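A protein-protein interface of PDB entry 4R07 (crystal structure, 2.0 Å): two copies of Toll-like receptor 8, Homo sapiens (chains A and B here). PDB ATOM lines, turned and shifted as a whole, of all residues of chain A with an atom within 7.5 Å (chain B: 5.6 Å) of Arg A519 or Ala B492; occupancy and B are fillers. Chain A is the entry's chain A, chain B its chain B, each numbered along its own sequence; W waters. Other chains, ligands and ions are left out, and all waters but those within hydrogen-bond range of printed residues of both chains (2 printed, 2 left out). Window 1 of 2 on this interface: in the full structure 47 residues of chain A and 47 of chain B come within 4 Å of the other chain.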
ATOM      1  N   PHE A 472      -3.669  -3.105 -24.496  1.00  0.00           N
ATOM      2  CA  PHE A 472      -4.195  -1.929 -25.230  1.00  0.00           C
ATOM      3  C   PHE A 472      -4.424  -2.221 -26.720  1.00  0.00           C
ATOM      4  O   PHE A 472      -5.126  -1.468 -27.424  1.00  0.00           O
ATOM      5  CB  PHE A 472      -3.310  -0.661 -25.008  1.00  0.00           C
ATOM      6  CG  PHE A 472      -2.003  -0.642 -25.787  1.00  0.00           C
ATOM      7  CD1 PHE A 472      -0.871  -1.267 -25.290  1.00  0.00           C
ATOM      8  CD2 PHE A 472      -1.928  -0.028 -27.018  1.00  0.00           C
ATOM      9  CE1 PHE A 472       0.317  -1.270 -25.993  1.00  0.00           C
ATOM     10  CE2 PHE A 472      -0.734   0.033 -27.711  1.00  0.00           C
ATOM     11  CZ  PHE A 472       0.393  -0.596 -27.200  1.00  0.00           C
ATOM     12  N   ALA A 492     -11.753  -2.526 -19.375  1.00  0.00           N
ATOM     13  CA  ALA A 492     -10.787  -1.599 -18.765  1.00  0.00           C
ATOM     14  C   ALA A 492      -9.345  -1.963 -19.039  1.00  0.00           C
ATOM     15  O   ALA A 492      -8.510  -2.032 -18.118  1.00  0.00           O
ATOM     16  CB  ALA A 492     -11.044  -1.442 -17.278  1.00  0.00           C
ATOM     17  N   ASN A 493      -9.050  -2.217 -20.317  1.00  0.00           N
ATOM     18  CA  ASN A 493      -7.683  -2.432 -20.750  1.00  0.00           C
ATOM     19  C   ASN A 493      -7.162  -1.283 -21.602  1.00  0.00           C
ATOM     20  O   ASN A 493      -6.064  -1.348 -22.114  1.00  0.00           O
ATOM     21  CB  ASN A 493      -7.568  -3.757 -21.534  1.00  0.00           C
ATOM     22  CG  ASN A 493      -7.309  -4.950 -20.623  1.00  0.00           C
ATOM     23  OD1 ASN A 493      -6.189  -5.173 -20.160  1.00  0.00           O
ATOM     24  ND2 ASN A 493      -8.368  -5.639 -20.264  1.00  0.00           N
ATOM     25  N   SER A 494      -7.970  -0.256 -21.756  1.00  0.00           N
ATOM     26  CA  SER A 494      -7.677   0.857 -22.650  1.00  0.00           C
ATOM     27  C   SER A 494      -7.370   0.374 -24.058  1.00  0.00           C
ATOM     28  O   SER A 494      -6.443   0.870 -24.706  1.00  0.00           O
ATOM     29  CB  SER A 494      -6.528   1.690 -22.104  1.00  0.00           C
ATOM     30  OG  SER A 494      -5.318   0.902 -22.149  1.00  0.00           O
ATOM     31  N   ASN A 495      -8.157  -0.591 -24.535  1.00  0.00           N
ATOM     32  CA  ASN A 495      -7.907  -1.172 -25.830  1.00  0.00           C
ATOM     33  C   ASN A 495      -8.439  -0.208 -26.900  1.00  0.00           C
ATOM     34  O   ASN A 495      -9.633   0.148 -26.947  1.00  0.00           O
ATOM     35  CB  ASN A 495      -8.523  -2.575 -25.915  1.00  0.00           C
ATOM     36  CG  ASN A 495      -8.252  -3.269 -27.239  1.00  0.00           C
ATOM     37  OD1 ASN A 495      -8.015  -2.646 -28.254  1.00  0.00           O
ATOM     38  ND2 ASN A 495      -8.338  -4.556 -27.226  1.00  0.00           N
ATOM     39  N   ALA A 496      -7.501   0.237 -27.727  1.00  0.00           N
ATOM     40  CA  ALA A 496      -7.739   1.234 -28.755  1.00  0.00           C
ATOM     41  C   ALA A 496      -7.762   0.672 -30.169  1.00  0.00           C
ATOM     42  O   ALA A 496      -7.749   1.450 -31.150  1.00  0.00           O
ATOM     43  CB  ALA A 496      -6.662   2.301 -28.657  1.00  0.00           C
ATOM     44  N   GLN A 497      -7.876  -0.648 -30.290  1.00  0.00           N
ATOM     45  CA  GLN A 497      -7.599  -1.274 -31.560  1.00  0.00           C
ATOM     46  C   GLN A 497      -8.779  -1.347 -32.459  1.00  0.00           C
ATOM     47  O   GLN A 497      -9.932  -1.128 -32.037  1.00  0.00           O
ATOM     48  CB  GLN A 497      -6.977  -2.653 -31.399  1.00  0.00           C
ATOM     49  CG  GLN A 497      -7.970  -3.780 -31.315  1.00  0.00           C
ATOM     50  CD  GLN A 497      -7.274  -5.091 -31.021  1.00  0.00           C
ATOM     51  OE1 GLN A 497      -7.301  -5.577 -29.890  1.00  0.00           O
ATOM     52  NE2 GLN A 497      -6.508  -5.571 -31.979  1.00  0.00           N
ATOM     53  N   VAL A 498      -8.455  -1.551 -33.741  1.00  0.00           N
ATOM     54  CA  VAL A 498      -9.438  -1.864 -34.754  1.00  0.00           C
ATOM     55  C   VAL A 498      -9.543  -3.372 -34.822  1.00  0.00           C
ATOM     56  O   VAL A 498      -8.649  -4.058 -35.340  1.00  0.00           O
ATOM     57  CB  VAL A 498      -9.023  -1.327 -36.147  1.00  0.00           C
ATOM     58  CG1 VAL A 498     -10.046  -1.738 -37.192  1.00  0.00           C
ATOM     59  CG2 VAL A 498      -8.852   0.196 -36.122  1.00  0.00           C
ATOM     60  N   LEU A 515     -16.334  -6.053 -23.100  1.00  0.00           N
ATOM     61  CA  LEU A 515     -15.299  -5.158 -23.605  1.00  0.00           C
ATOM     62  C   LEU A 515     -15.590  -3.730 -23.179  1.00  0.00           C
ATOM     63  O   LEU A 515     -15.244  -2.788 -23.895  1.00  0.00           O
ATOM     64  CB  LEU A 515     -15.265  -5.219 -25.131  1.00  0.00           C
ATOM     65  CG  LEU A 515     -14.519  -6.400 -25.734  1.00  0.00           C
ATOM     66  CD1 LEU A 515     -14.843  -6.527 -27.209  1.00  0.00           C
ATOM     67  CD2 LEU A 515     -13.032  -6.186 -25.573  1.00  0.00           C
ATOM     68  N   THR A 516     -16.234  -3.560 -22.024  1.00  0.00           N
ATOM     69  CA  THR A 516     -16.611  -2.251 -21.567  1.00  0.00           C
ATOM     70  C   THR A 516     -15.361  -1.467 -21.211  1.00  0.00           C
ATOM     71  O   THR A 516     -14.319  -2.063 -20.895  1.00  0.00           O
ATOM     72  CB  THR A 516     -17.481  -2.317 -20.266  1.00  0.00           C
ATOM     73  OG1 THR A 516     -16.718  -2.922 -19.224  1.00  0.00           O
ATOM     74  CG2 THR A 516     -18.717  -3.101 -20.496  1.00  0.00           C
ATOM     75  N   ASN A 517     -15.500  -0.147 -21.156  1.00  0.00           N
ATOM     76  CA  ASN A 517     -14.443   0.727 -20.611  1.00  0.00           C
ATOM     77  C   ASN A 517     -13.135   0.552 -21.327  1.00  0.00           C
ATOM     78  O   ASN A 517     -12.086   0.340 -20.706  1.00  0.00           O
ATOM     79  CB  ASN A 517     -14.253   0.454 -19.138  1.00  0.00           C
ATOM     80  CG  ASN A 517     -15.477   0.766 -18.362  1.00  0.00           C
ATOM     81  OD1 ASN A 517     -16.307  -0.094 -18.162  1.00  0.00           O
ATOM     82  ND2 ASN A 517     -15.610   1.991 -17.918  1.00  0.00           N
ATOM     83  N   ASN A 518     -13.211   0.512 -22.641  1.00  0.00           N
ATOM     84  CA  ASN A 518     -12.040   0.523 -23.473  1.00  0.00           C
ATOM     85  C   ASN A 518     -12.122   1.726 -24.388  1.00  0.00           C
ATOM     86  O   ASN A 518     -12.919   2.652 -24.123  1.00  0.00           O
ATOM     87  CB  ASN A 518     -11.927  -0.775 -24.278  1.00  0.00           C
ATOM     88  CG  ASN A 518     -11.364  -1.923 -23.453  1.00  0.00           C
ATOM     89  OD1 ASN A 518     -10.205  -1.860 -23.000  1.00  0.00           O
ATOM     90  ND2 ASN A 518     -12.235  -2.882 -23.096  1.00  0.00           N
ATOM     91  N   ARG A 519     -11.297   1.750 -25.428  1.00  0.00           N
ATOM     92  CA  ARG A 519     -11.379   2.835 -26.373  1.00  0.00           C
ATOM     93  C   ARG A 519     -11.355   2.335 -27.797  1.00  0.00           C
ATOM     94  O   ARG A 519     -10.618   2.826 -28.657  1.00  0.00           O
ATOM     95  CB  ARG A 519     -10.301   3.892 -26.096  1.00  0.00           C
ATOM     96  CG  ARG A 519      -8.925   3.348 -25.846  1.00  0.00           C
ATOM     97  CD  ARG A 519      -7.924   4.479 -25.903  1.00  0.00           C
ATOM     98  NE  ARG A 519      -7.706   5.110 -24.622  1.00  0.00           N
ATOM     99  CZ  ARG A 519      -6.758   6.021 -24.386  1.00  0.00           C
ATOM    100  NH1 ARG A 519      -5.932   6.430 -25.341  1.00  0.00           N
ATOM    101  NH2 ARG A 519      -6.615   6.495 -23.168  1.00  0.00           N
ATOM    102  N   LEU A 520     -12.221   1.381 -28.065  1.00  0.00           N
ATOM    103  CA  LEU A 520     -12.162   0.676 -29.339  1.00  0.00           C
ATOM    104  C   LEU A 520     -12.394   1.587 -30.571  1.00  0.00           C
ATOM    105  O   LEU A 520     -13.252   2.461 -30.587  1.00  0.00           O
ATOM    106  CB  LEU A 520     -13.145  -0.491 -29.302  1.00  0.00           C
ATOM    107  CG  LEU A 520     -12.748  -1.628 -28.344  1.00  0.00           C
ATOM    108  CD1 LEU A 520     -13.934  -2.560 -28.115  1.00  0.00           C
ATOM    109  CD2 LEU A 520     -11.577  -2.419 -28.892  1.00  0.00           C
ATOM    110  N   ASP A 521     -11.615   1.348 -31.613  1.00  0.00           N
ATOM    111  CA  ASP A 521     -11.740   2.077 -32.875  1.00  0.00           C
ATOM    112  C   ASP A 521     -12.504   1.250 -33.911  1.00  0.00           C
ATOM    113  O   ASP A 521     -12.000   0.255 -34.454  1.00  0.00           O
ATOM    114  CB  ASP A 521     -10.363   2.389 -33.399  1.00  0.00           C
ATOM    115  CG  ASP A 521     -10.383   3.319 -34.600  1.00  0.00           C
ATOM    116  OD1 ASP A 521     -11.418   3.959 -34.836  1.00  0.00           O
ATOM    117  OD2 ASP A 521      -9.317   3.476 -35.227  1.00  0.00           O
ATOM    118  N   PHE A 522     -13.757   1.612 -34.124  1.00  0.00           N
ATOM    119  CA  PHE A 522     -14.604   0.797 -34.948  1.00  0.00           C
ATOM    120  C   PHE A 522     -14.425   1.123 -36.438  1.00  0.00           C
ATOM    121  O   PHE A 522     -15.296   1.704 -37.069  1.00  0.00           O
ATOM    122  CB  PHE A 522     -16.037   0.917 -34.513  1.00  0.00           C
ATOM    123  CG  PHE A 522     -16.281   0.306 -33.174  1.00  0.00           C
ATOM    124  CD1 PHE A 522     -16.262  -1.077 -33.017  1.00  0.00           C
ATOM    125  CD2 PHE A 522     -16.362   1.095 -32.055  1.00  0.00           C
ATOM    126  CE1 PHE A 522     -16.399  -1.651 -31.768  1.00  0.00           C
ATOM    127  CE2 PHE A 522     -16.565   0.524 -30.803  1.00  0.00           C
ATOM    128  CZ  PHE A 522     -16.556  -0.845 -30.657  1.00  0.00           C
ATOM    129  N   TYR A 541     -19.221   2.197 -22.449  1.00  0.00           N
ATOM    130  CA  TYR A 541     -18.058   3.085 -22.192  1.00  0.00           C
ATOM    131  C   TYR A 541     -16.871   2.894 -23.095  1.00  0.00           C
ATOM    132  O   TYR A 541     -15.753   2.668 -22.610  1.00  0.00           O
ATOM    133  CB  TYR A 541     -17.585   2.918 -20.753  1.00  0.00           C
ATOM    134  CG  TYR A 541     -18.668   3.212 -19.738  1.00  0.00           C
ATOM    135  CD1 TYR A 541     -18.925   4.527 -19.299  1.00  0.00           C
ATOM    136  CD2 TYR A 541     -19.420   2.195 -19.200  1.00  0.00           C
ATOM    137  CE1 TYR A 541     -19.938   4.782 -18.385  1.00  0.00           C
ATOM    138  CE2 TYR A 541     -20.438   2.452 -18.293  1.00  0.00           C
ATOM    139  CZ  TYR A 541     -20.687   3.734 -17.897  1.00  0.00           C
ATOM    140  OH  TYR A 541     -21.692   3.940 -17.010  1.00  0.00           O
ATOM    141  N   ASN A 542     -17.129   2.875 -24.404  1.00  0.00           N
ATOM    142  CA  ASN A 542     -16.087   3.022 -25.390  1.00  0.00           C
ATOM    143  C   ASN A 542     -16.280   4.320 -26.182  1.00  0.00           C
ATOM    144  O   ASN A 542     -16.141   4.342 -27.409  1.00  0.00           O
ATOM    145  CB  ASN A 542     -16.034   1.832 -26.348  1.00  0.00           C
ATOM    146  CG  ASN A 542     -15.363   0.620 -25.737  1.00  0.00           C
ATOM    147  OD1 ASN A 542     -14.202   0.361 -25.977  1.00  0.00           O
ATOM    148  ND2 ASN A 542     -16.103  -0.110 -24.916  1.00  0.00           N
ATOM    149  N   SER A 543     -16.613   5.383 -25.499  1.00  0.00           N
ATOM    150  CA  SER A 543     -16.867   6.618 -26.172  1.00  0.00           C
ATOM    151  C   SER A 543     -15.664   7.262 -26.903  1.00  0.00           C
ATOM    152  O   SER A 543     -15.857   8.061 -27.757  1.00  0.00           O
ATOM    153  CB  SER A 543     -17.605   7.583 -25.287  1.00  0.00           C
ATOM    154  OG  SER A 543     -16.772   8.027 -24.310  1.00  0.00           O
ATOM    155  N   HIS A 544     -14.457   6.908 -26.504  1.00  0.00           N
ATOM    156  CA  HIS A 544     -13.235   7.595 -26.969  1.00  0.00           C
ATOM    157  C   HIS A 544     -13.291   8.072 -28.424  1.00  0.00           C
ATOM    158  O   HIS A 544     -13.149   9.290 -28.685  1.00  0.00           O
ATOM    159  CB  HIS A 544     -12.055   6.678 -26.785  1.00  0.00           C
ATOM    160  CG  HIS A 544     -10.718   7.296 -27.095  1.00  0.00           C
ATOM    161  ND1 HIS A 544      -9.811   7.619 -26.112  1.00  0.00           N
ATOM    162  CD2 HIS A 544     -10.120   7.608 -28.271  1.00  0.00           C
ATOM    163  CE1 HIS A 544      -8.703   8.083 -26.671  1.00  0.00           C
ATOM    164  NE2 HIS A 544      -8.875   8.116 -27.976  1.00  0.00           N
ATOM    165  N   TYR A 545     -13.526   7.135 -29.357  1.00  0.00           N
ATOM    166  CA  TYR A 545     -13.485   7.442 -30.793  1.00  0.00           C
ATOM    167  C   TYR A 545     -14.835   7.859 -31.350  1.00  0.00           C
ATOM    168  O   TYR A 545     -14.896   8.632 -32.307  1.00  0.00           O
ATOM    169  CB  TYR A 545     -12.903   6.283 -31.600  1.00  0.00           C
ATOM    170  CG  TYR A 545     -11.417   6.135 -31.447  1.00  0.00           C
ATOM    171  CD1 TYR A 545     -10.880   5.072 -30.753  1.00  0.00           C
ATOM    172  CD2 TYR A 545     -10.549   7.089 -31.947  1.00  0.00           C
ATOM    173  CE1 TYR A 545      -9.519   4.917 -30.635  1.00  0.00           C
ATOM    174  CE2 TYR A 545      -9.169   6.963 -31.805  1.00  0.00           C
ATOM    175  CZ  TYR A 545      -8.661   5.917 -31.092  1.00  0.00           C
ATOM    176  OH  TYR A 545      -7.287   5.733 -30.942  1.00  0.00           O
ATOM    177  N   PHE A 546     -15.910   7.492 -30.661  1.00  0.00           N
ATOM    178  CA  PHE A 546     -17.227   7.892 -31.079  1.00  0.00           C
ATOM    179  C   PHE A 546     -17.391   9.381 -30.940  1.00  0.00           C
ATOM    180  O   PHE A 546     -18.264   9.951 -31.590  1.00  0.00           O
ATOM    181  CB  PHE A 546     -18.340   7.214 -30.261  1.00  0.00           C
ATOM    182  CG  PHE A 546     -18.608   5.789 -30.624  1.00  0.00           C
ATOM    183  CD1 PHE A 546     -19.069   5.439 -31.899  1.00  0.00           C
ATOM    184  CD2 PHE A 546     -18.506   4.796 -29.677  1.00  0.00           C
ATOM    185  CE1 PHE A 546     -19.337   4.109 -32.212  1.00  0.00           C
ATOM    186  CE2 PHE A 546     -18.754   3.469 -29.979  1.00  0.00           C
ATOM    187  CZ  PHE A 546     -19.155   3.123 -31.259  1.00  0.00           C
ATOM    188  N   SER B 467      -1.460  13.768 -25.200  1.00  0.00           N
ATOM    189  CA  SER B 467      -2.655  13.240 -24.571  1.00  0.00           C
ATOM    190  C   SER B 467      -3.335  12.262 -25.522  1.00  0.00           C
ATOM    191  O   SER B 467      -3.106  12.306 -26.717  1.00  0.00           O
ATOM    192  CB  SER B 467      -3.617  14.370 -24.242  1.00  0.00           C
ATOM    193  OG  SER B 467      -3.864  15.181 -25.384  1.00  0.00           O
ATOM    194  N   LEU B 468      -4.169  11.384 -24.971  1.00  0.00           N
ATOM    195  CA  LEU B 468      -5.007  10.498 -25.749  1.00  0.00           C
ATOM    196  C   LEU B 468      -4.175   9.622 -26.688  1.00  0.00           C
ATOM    197  O   LEU B 468      -4.524   9.428 -27.854  1.00  0.00           O
ATOM    198  CB  LEU B 468      -6.068  11.311 -26.494  1.00  0.00           C
ATOM    199  CG  LEU B 468      -7.034  12.032 -25.538  1.00  0.00           C
ATOM    200  CD1 LEU B 468      -7.720  13.231 -26.180  1.00  0.00           C
ATOM    201  CD2 LEU B 468      -8.074  11.086 -24.911  1.00  0.00           C
ATOM    202  N   ASN B 469      -3.050   9.129 -26.173  1.00  0.00           N
ATOM    203  CA  ASN B 469      -2.296   8.068 -26.806  1.00  0.00           C
ATOM    204  C   ASN B 469      -2.334   6.846 -25.891  1.00  0.00           C
ATOM    205  O   ASN B 469      -3.137   6.784 -24.939  1.00  0.00           O
ATOM    206  CB  ASN B 469      -0.849   8.534 -27.098  1.00  0.00           C
ATOM    207  CG  ASN B 469      -0.770   9.503 -28.288  1.00  0.00           C
ATOM    208  OD1 ASN B 469      -0.818   9.105 -29.458  1.00  0.00           O
ATOM    209  ND2 ASN B 469      -0.820  10.771 -27.983  1.00  0.00           N
ATOM    210  N   SER B 470      -1.391   5.936 -26.104  1.00  0.00           N
ATOM    211  CA  SER B 470      -1.313   4.693 -25.361  1.00  0.00           C
ATOM    212  C   SER B 470       0.029   4.506 -24.693  1.00  0.00           C
ATOM    213  O   SER B 470       0.570   3.417 -24.655  1.00  0.00           O
ATOM    214  CB  SER B 470      -1.602   3.516 -26.292  1.00  0.00           C
ATOM    215  OG  SER B 470      -2.927   3.581 -26.791  1.00  0.00           O
ATOM    216  N   LEU B 490       0.303  14.587 -20.711  1.00  0.00           N
ATOM    217  CA  LEU B 490       0.210  13.147 -20.837  1.00  0.00           C
ATOM    218  C   LEU B 490      -1.147  12.623 -20.414  1.00  0.00           C
ATOM    219  O   LEU B 490      -1.323  11.416 -20.127  1.00  0.00           O
ATOM    220  CB  LEU B 490       1.321  12.475 -20.045  1.00  0.00           C
ATOM    221  CG  LEU B 490       2.729  12.662 -20.549  1.00  0.00           C
ATOM    222  CD1 LEU B 490       3.721  12.106 -19.533  1.00  0.00           C
ATOM    223  CD2 LEU B 490       2.943  11.930 -21.855  1.00  0.00           C
ATOM    224  N   SER B 491      -2.140  13.488 -20.479  1.00  0.00           N
ATOM    225  CA  SER B 491      -3.500  13.073 -20.096  1.00  0.00           C
ATOM    226  C   SER B 491      -4.020  11.886 -20.901  1.00  0.00           C
ATOM    227  O   SER B 491      -3.633  11.703 -22.044  1.00  0.00           O
ATOM    228  CB  SER B 491      -4.462  14.242 -20.211  1.00  0.00           C
ATOM    229  OG  SER B 491      -5.764  13.828 -19.852  1.00  0.00           O
ATOM    230  N   ALA B 492      -4.760  10.988 -20.244  1.00  0.00           N
ATOM    231  CA  ALA B 492      -5.523   9.951 -20.940  1.00  0.00           C
ATOM    232  C   ALA B 492      -4.636   9.044 -21.819  1.00  0.00           C
ATOM    233  O   ALA B 492      -4.918   8.767 -22.963  1.00  0.00           O
ATOM    234  CB  ALA B 492      -6.669  10.570 -21.726  1.00  0.00           C
ATOM    235  N   ASN B 493      -3.581   8.552 -21.206  1.00  0.00           N
ATOM    236  CA  ASN B 493      -2.718   7.534 -21.773  1.00  0.00           C
ATOM    237  C   ASN B 493      -2.893   6.179 -21.091  1.00  0.00           C
ATOM    238  O   ASN B 493      -2.170   5.255 -21.364  1.00  0.00           O
ATOM    239  CB  ASN B 493      -1.302   8.003 -21.669  1.00  0.00           C
ATOM    240  CG  ASN B 493      -0.877   8.801 -22.903  1.00  0.00           C
ATOM    241  OD1 ASN B 493      -0.616   8.233 -23.976  1.00  0.00           O
ATOM    242  ND2 ASN B 493      -0.925  10.120 -22.787  1.00  0.00           N
ATOM    243  N   SER B 494      -3.837   6.090 -20.163  1.00  0.00           N
ATOM    244  CA  SER B 494      -3.934   4.911 -19.253  1.00  0.00           C
ATOM    245  C   SER B 494      -2.570   4.465 -18.708  1.00  0.00           C
ATOM    246  O   SER B 494      -2.243   3.274 -18.635  1.00  0.00           O
ATOM    247  CB  SER B 494      -4.640   3.774 -19.980  1.00  0.00           C
ATOM    248  OG  SER B 494      -3.789   3.294 -21.035  1.00  0.00           O
ATOM    249  N   LEU B 515      -1.122  15.117 -15.962  1.00  0.00           N
ATOM    250  CA  LEU B 515      -1.248  13.643 -15.922  1.00  0.00           C
ATOM    251  C   LEU B 515      -2.661  13.164 -15.576  1.00  0.00           C
ATOM    252  O   LEU B 515      -2.859  12.071 -15.030  1.00  0.00           O
ATOM    253  CB  LEU B 515      -0.246  13.109 -14.866  1.00  0.00           C
ATOM    254  CG  LEU B 515       1.187  12.940 -15.343  1.00  0.00           C
ATOM    255  CD1 LEU B 515       2.153  12.764 -14.194  1.00  0.00           C
ATOM    256  CD2 LEU B 515       1.330  11.751 -16.292  1.00  0.00           C
ATOM    257  N   THR B 516      -3.662  13.956 -15.924  1.00  0.00           N
ATOM    258  CA  THR B 516      -5.037  13.624 -15.636  1.00  0.00           C
ATOM    259  C   THR B 516      -5.487  12.373 -16.423  1.00  0.00           C
ATOM    260  O   THR B 516      -4.906  12.043 -17.430  1.00  0.00           O
ATOM    261  CB  THR B 516      -5.975  14.754 -16.007  1.00  0.00           C
ATOM    262  OG1 THR B 516      -5.971  14.916 -17.408  1.00  0.00           O
ATOM    263  CG2 THR B 516      -5.562  16.087 -15.363  1.00  0.00           C
ATOM    264  N   ASN B 517      -6.480  11.666 -15.919  1.00  0.00           N
ATOM    265  CA  ASN B 517      -7.129  10.559 -16.657  1.00  0.00           C
ATOM    266  C   ASN B 517      -6.146   9.431 -17.008  1.00  0.00           C
ATOM    267  O   ASN B 517      -6.057   8.952 -18.146  1.00  0.00           O
ATOM    268  CB  ASN B 517      -7.870  11.061 -17.887  1.00  0.00           C
ATOM    269  CG  ASN B 517      -8.989  12.011 -17.537  1.00  0.00           C
ATOM    270  OD1 ASN B 517     -10.134  11.592 -17.284  1.00  0.00           O
ATOM    271  ND2 ASN B 517      -8.657  13.287 -17.405  1.00  0.00           N
ATOM    272  N   ASN B 518      -5.340   9.081 -16.026  1.00  0.00           N
ATOM    273  CA  ASN B 518      -4.474   7.950 -16.122  1.00  0.00           C
ATOM    274  C   ASN B 518      -4.815   6.999 -14.999  1.00  0.00           C
ATOM    275  O   ASN B 518      -5.913   7.044 -14.459  1.00  0.00           O
ATOM    276  CB  ASN B 518      -3.013   8.382 -16.132  1.00  0.00           C
ATOM    277  CG  ASN B 518      -2.578   8.920 -17.478  1.00  0.00           C
ATOM    278  OD1 ASN B 518      -2.578   8.196 -18.488  1.00  0.00           O
ATOM    279  ND2 ASN B 518      -2.257  10.218 -17.522  1.00  0.00           N
HETATM  280  O   HOH W   1      -6.622   7.025 -19.888  1.00  0.00           O
HETATM  281  O   HOH W   2      -4.567   3.051 -24.822  1.00  0.00           O
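The side-chain hydroxyl (OG) of Ser B494 is in hydrogen-bond range of the side-chain hydroxyl (OG) of Ser A494 (3.0 Å). The guanidinium group (NH1) of Arg A519 sits at hydrogen-bond distance from the backbone carbonyl oxygen (O) of Asn B469 (2.8 Å). O of Ala B492 lies within hydrogen-bond range of NH2 of Arg A519.
The backbone carbonyl oxygen (O) of Phe A472 sits close to the side-chain amide oxygen (OD1) of Asn A495 (3.2 Å). The backbone NH (N) of Ser A494 lies within hydrogen-bond range of the side-chain amide oxygen (OD1) of Asn A518 (3.0 Å). The side-chain amide oxygen (OD1) of Asn A542 is in hydrogen-bond range of the backbone NH (N) of Arg A519, 3.3 Å away. N of Leu B468 lies within hydrogen-bond range of O of Ser B491, at 3.0 Å. The backbone carbonyl oxygen (O) of Ala B492 sits close to the backbone NH (N) of Leu B468. N of Ser B494 lies within hydrogen-bond range of OD1 of Asn B518 (3.0 Å).
Phe A472 touches Ser B470. Arg A519 touches Leu B468. CE1 of His A544 touches CD2 of Leu B468, 3.5 Å away.
Of the printed residues of chain B, Arg A519 touches Leu B468, Asn B469 and Ala B492. Printed residues of chain A within 4 Å of Ala B492: Arg A519. Of the printed residues of chain A, Leu B468 touches Arg A519 and His A544. Printed residues of chain B within 4 Å of His A544: Leu B468. Ala A496 touches none of the printed residues of chain B. Thr A516 touches none of the printed residues of chain B.
Hydrophobic or aromatic side chains of chain B within 4 Å of the printed part of chain A: Leu B468. Hydrophobic or aromatic side chains of chain A that line the printed part of chain B: Phe A472 and His A544. Among the printed residues, 6 pairs touch across the chains.
Ser A494 touches its own counterpart, Ser B494. Positions printed for both chains: 492, 493, 494, 515, 516, 517 and 518. Of the 6 pairs that touch across the chains among the printed residues, 1 has its exchanged pair printed and touching as well.
Water W2 lies within hydrogen-bond range of the side-chain hydroxyl (OG) of Ser B470 (2.6 Å) and the backbone carbonyl oxygen (O) of Ser A494 (2.9 Å). Water W1 lies within hydrogen-bond range of O of Asn B517, N of Ser B494 and NH2 of Arg A519.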
